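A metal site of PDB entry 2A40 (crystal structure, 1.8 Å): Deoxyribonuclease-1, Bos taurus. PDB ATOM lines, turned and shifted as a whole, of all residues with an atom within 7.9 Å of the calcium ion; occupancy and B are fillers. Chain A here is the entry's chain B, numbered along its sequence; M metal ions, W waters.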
ATOM      1  N   ALA A 200     -27.560  14.309 -12.830  1.00  0.00           N
ATOM      2  CA  ALA A 200     -26.389  13.997 -11.986  1.00  0.00           C
ATOM      3  C   ALA A 200     -25.003  14.194 -12.626  1.00  0.00           C
ATOM      4  O   ALA A 200     -24.769  13.836 -13.786  1.00  0.00           O
ATOM      5  CB  ALA A 200     -26.499  12.598 -11.428  1.00  0.00           C
ATOM      6  N   ASP A 201     -24.047  14.681 -11.831  1.00  0.00           N
ATOM      7  CA  ASP A 201     -22.665  14.803 -12.306  1.00  0.00           C
ATOM      8  C   ASP A 201     -21.917  13.581 -11.763  1.00  0.00           C
ATOM      9  O   ASP A 201     -21.687  13.473 -10.564  1.00  0.00           O
ATOM     10  CB  ASP A 201     -22.010  16.097 -11.803  1.00  0.00           C
ATOM     11  CG  ASP A 201     -20.558  16.206 -12.213  1.00  0.00           C
ATOM     12  OD1 ASP A 201     -20.155  15.526 -13.197  1.00  0.00           O
ATOM     13  OD2 ASP A 201     -19.810  16.957 -11.573  1.00  0.00           O
ATOM     14  N   THR A 202     -21.541  12.670 -12.644  1.00  0.00           N
ATOM     15  CA  THR A 202     -20.745  11.549 -12.168  1.00  0.00           C
ATOM     16  C   THR A 202     -19.285  11.590 -12.609  1.00  0.00           C
ATOM     17  O   THR A 202     -18.592  10.590 -12.484  1.00  0.00           O
ATOM     18  CB  THR A 202     -21.369  10.179 -12.594  1.00  0.00           C
ATOM     19  OG1 THR A 202     -21.111   9.936 -13.988  1.00  0.00           O
ATOM     20  CG2 THR A 202     -22.914  10.181 -12.348  1.00  0.00           C
ATOM     21  N   THR A 203     -18.823  12.730 -13.128  1.00  0.00           N
ATOM     22  CA  THR A 203     -17.387  12.928 -13.472  1.00  0.00           C
ATOM     23  C   THR A 203     -16.621  13.699 -12.434  1.00  0.00           C
ATOM     24  O   THR A 203     -17.115  14.702 -11.922  1.00  0.00           O
ATOM     25  CB  THR A 203     -17.196  13.646 -14.832  1.00  0.00           C
ATOM     26  OG1 THR A 203     -17.676  15.012 -14.804  1.00  0.00           O
ATOM     27  CG2 THR A 203     -17.899  12.833 -15.950  1.00  0.00           C
ATOM     28  N   ALA A 204     -15.401  13.239 -12.112  1.00  0.00           N
ATOM     29  CA  ALA A 204     -14.519  14.008 -11.221  1.00  0.00           C
ATOM     30  C   ALA A 204     -13.898  15.142 -11.975  1.00  0.00           C
ATOM     31  O   ALA A 204     -13.346  16.072 -11.376  1.00  0.00           O
ATOM     32  CB  ALA A 204     -13.420  13.126 -10.658  1.00  0.00           C
ATOM     33  N   THR A 205     -13.993  15.100 -13.296  1.00  0.00           N
ATOM     34  CA  THR A 205     -13.482  16.207 -14.127  1.00  0.00           C
ATOM     35  C   THR A 205     -14.488  17.373 -14.241  1.00  0.00           C
ATOM     36  O   THR A 205     -15.602  17.303 -13.715  1.00  0.00           O
ATOM     37  CB  THR A 205     -13.232  15.725 -15.550  1.00  0.00           C
ATOM     38  OG1 THR A 205     -14.471  15.388 -16.142  1.00  0.00           O
ATOM     39  CG2 THR A 205     -12.368  14.471 -15.559  1.00  0.00           C
ATOM     40  N   SER A 206     -14.105  18.415 -14.968  1.00  0.00           N
ATOM     41  CA  SER A 206     -14.950  19.610 -15.120  1.00  0.00           C
ATOM     42  C   SER A 206     -16.163  19.446 -16.058  1.00  0.00           C
ATOM     43  O   SER A 206     -16.931  20.354 -16.270  1.00  0.00           O
ATOM     44  CB  SER A 206     -14.108  20.790 -15.580  1.00  0.00           C
ATOM     45  OG  SER A 206     -13.605  20.538 -16.877  1.00  0.00           O
ATOM     46  N   THR A 207     -16.312  18.294 -16.671  1.00  0.00           N
ATOM     47  CA  THR A 207     -17.572  18.072 -17.395  1.00  0.00           C
ATOM     48  C   THR A 207     -18.721  17.867 -16.396  1.00  0.00           C
ATOM     49  O   THR A 207     -18.495  17.434 -15.271  1.00  0.00           O
ATOM     50  CB  THR A 207     -17.485  16.855 -18.303  1.00  0.00           C
ATOM     51  OG1 THR A 207     -17.353  15.677 -17.489  1.00  0.00           O
ATOM     52  CG2 THR A 207     -16.296  16.943 -19.226  1.00  0.00           C
ATOM     53  N   ASN A 208     -19.942  18.182 -16.832  1.00  0.00           N
ATOM     54  CA  ASN A 208     -21.129  17.904 -16.056  1.00  0.00           C
ATOM     55  C   ASN A 208     -21.907  16.853 -16.828  1.00  0.00           C
ATOM     56  O   ASN A 208     -22.674  17.193 -17.733  1.00  0.00           O
ATOM     57  CB  ASN A 208     -21.985  19.154 -15.897  1.00  0.00           C
ATOM     58  CG  ASN A 208     -23.312  18.824 -15.263  1.00  0.00           C
ATOM     59  OD1 ASN A 208     -23.387  17.879 -14.463  1.00  0.00           O
ATOM     60  ND2 ASN A 208     -24.369  19.531 -15.662  1.00  0.00           N
ATOM     61  N   CYS A 209     -21.651  15.596 -16.495  1.00  0.00           N
ATOM     62  CA  CYS A 209     -22.241  14.475 -17.252  1.00  0.00           C
ATOM     63  C   CYS A 209     -22.675  13.328 -16.376  1.00  0.00           C
ATOM     64  O   CYS A 209     -21.910  12.867 -15.543  1.00  0.00           O
ATOM     65  CB  CYS A 209     -21.240  13.913 -18.242  1.00  0.00           C
ATOM     66  SG  CYS A 209     -20.671  15.138 -19.456  1.00  0.00           S
ATOM     67  N   ASP A 234     -19.199  11.967  -4.419  1.00  0.00           N
ATOM     68  CA  ASP A 234     -18.144  12.943  -4.722  1.00  0.00           C
ATOM     69  C   ASP A 234     -17.013  12.806  -3.711  1.00  0.00           C
ATOM     70  O   ASP A 234     -17.042  13.444  -2.647  1.00  0.00           O
ATOM     71  CB  ASP A 234     -18.711  14.388  -4.737  1.00  0.00           C
ATOM     72  CG  ASP A 234     -17.635  15.446  -5.027  1.00  0.00           C
ATOM     73  OD1 ASP A 234     -16.446  15.077  -5.040  1.00  0.00           O
ATOM     74  OD2 ASP A 234     -17.990  16.645  -5.226  1.00  0.00           O
ATOM     75  N   ASN A 243      -8.439  19.027  -6.544  1.00  0.00           N
ATOM     76  CA  ASN A 243      -8.962  18.400  -7.752  1.00  0.00           C
ATOM     77  C   ASN A 243      -7.917  17.508  -8.380  1.00  0.00           C
ATOM     78  O   ASN A 243      -8.253  16.441  -8.915  1.00  0.00           O
ATOM     79  CB  ASN A 243      -9.495  19.416  -8.774  1.00  0.00           C
ATOM     80  CG  ASN A 243     -10.179  18.740  -9.978  1.00  0.00           C
ATOM     81  OD1 ASN A 243     -11.170  17.985  -9.842  1.00  0.00           O
ATOM     82  ND2 ASN A 243      -9.646  19.005 -11.159  1.00  0.00           N
ATOM     83  N   ASP A 251     -11.215   9.752 -12.983  1.00  0.00           N
ATOM     84  CA  ASP A 251     -11.955  10.841 -13.612  1.00  0.00           C
ATOM     85  C   ASP A 251     -13.462  10.655 -13.468  1.00  0.00           C
ATOM     86  O   ASP A 251     -14.218  11.481 -13.977  1.00  0.00           O
ATOM     87  CB  ASP A 251     -11.571  11.017 -15.075  1.00  0.00           C
ATOM     88  CG  ASP A 251     -11.735   9.741 -15.882  1.00  0.00           C
ATOM     89  OD1 ASP A 251     -11.777   8.658 -15.269  1.00  0.00           O
ATOM     90  OD2 ASP A 251     -11.778   9.815 -17.131  1.00  0.00           O
ATOM     91  N   HIS A 252     -13.886   9.581 -12.803  1.00  0.00           N
ATOM     92  CA  HIS A 252     -15.299   9.354 -12.454  1.00  0.00           C
ATOM     93  C   HIS A 252     -15.531   9.225 -10.937  1.00  0.00           C
ATOM     94  O   HIS A 252     -14.666   8.767 -10.207  1.00  0.00           O
ATOM     95  CB  HIS A 252     -15.799   8.039 -13.047  1.00  0.00           C
ATOM     96  CG  HIS A 252     -15.836   7.997 -14.550  1.00  0.00           C
ATOM     97  ND1 HIS A 252     -17.011   7.937 -15.272  1.00  0.00           N
ATOM     98  CD2 HIS A 252     -14.834   7.980 -15.462  1.00  0.00           C
ATOM     99  CE1 HIS A 252     -16.733   7.900 -16.561  1.00  0.00           C
ATOM    100  NE2 HIS A 252     -15.423   7.940 -16.706  1.00  0.00           N
ATOM    101  N   TYR A 253     -16.745   9.548 -10.500  1.00  0.00           N
ATOM    102  CA  TYR A 253     -17.171   9.243  -9.127  1.00  0.00           C
ATOM    103  C   TYR A 253     -17.884   7.912  -9.165  1.00  0.00           C
ATOM    104  O   TYR A 253     -18.491   7.575 -10.201  1.00  0.00           O
ATOM    105  CB  TYR A 253     -18.188  10.288  -8.616  1.00  0.00           C
ATOM    106  CG  TYR A 253     -17.717  11.722  -8.589  1.00  0.00           C
ATOM    107  CD1 TYR A 253     -16.423  12.054  -8.165  1.00  0.00           C
ATOM    108  CD2 TYR A 253     -18.558  12.754  -8.994  1.00  0.00           C
ATOM    109  CE1 TYR A 253     -15.979  13.417  -8.155  1.00  0.00           C
ATOM    110  CE2 TYR A 253     -18.133  14.075  -9.007  1.00  0.00           C
ATOM    111  CZ  TYR A 253     -16.851  14.402  -8.580  1.00  0.00           C
ATOM    112  OH  TYR A 253     -16.454  15.712  -8.565  1.00  0.00           O
HETATM  113 CA    CA M   1     -17.889  16.742 -13.037  1.00  0.00          CA
HETATM  114  O   HOH W   1     -16.903  17.412 -10.860  1.00  0.00           O
HETATM  115  O   HOH W   2     -18.247  19.126 -12.879  1.00  0.00           O
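The side-chain hydroxyl (OG1) of Thr 207 sits at hydrogen-bond distance from the side-chain hydroxyl (OG1) of Thr 205, 3.2 Å away.
Four residues have an atom within 4 Å of the calcium ion: Asp 201, Thr 203, Thr 205 and Thr 207.
The nearest printed residue that does not touch the calcium ion is Ala 204 (4.4 Å).
The calcium ion is bound by water W2 (2.4 Å), the backbone carbonyl oxygen (O) of Thr 207 (2.4 Å), the side-chain carboxylate (OD2) of Asp 201 (2.4 Å), the backbone carbonyl oxygen (O) of Thr 205 (2.5 Å), the backbone carbonyl oxygen (O) of Thr 203 (2.5 Å), water W1 (2.5 Å), the side-chain hydroxyl (OG1) of Thr 203 (2.5 Å) and the side-chain carboxylate (OD1) of Asp 201 (2.6 Å).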
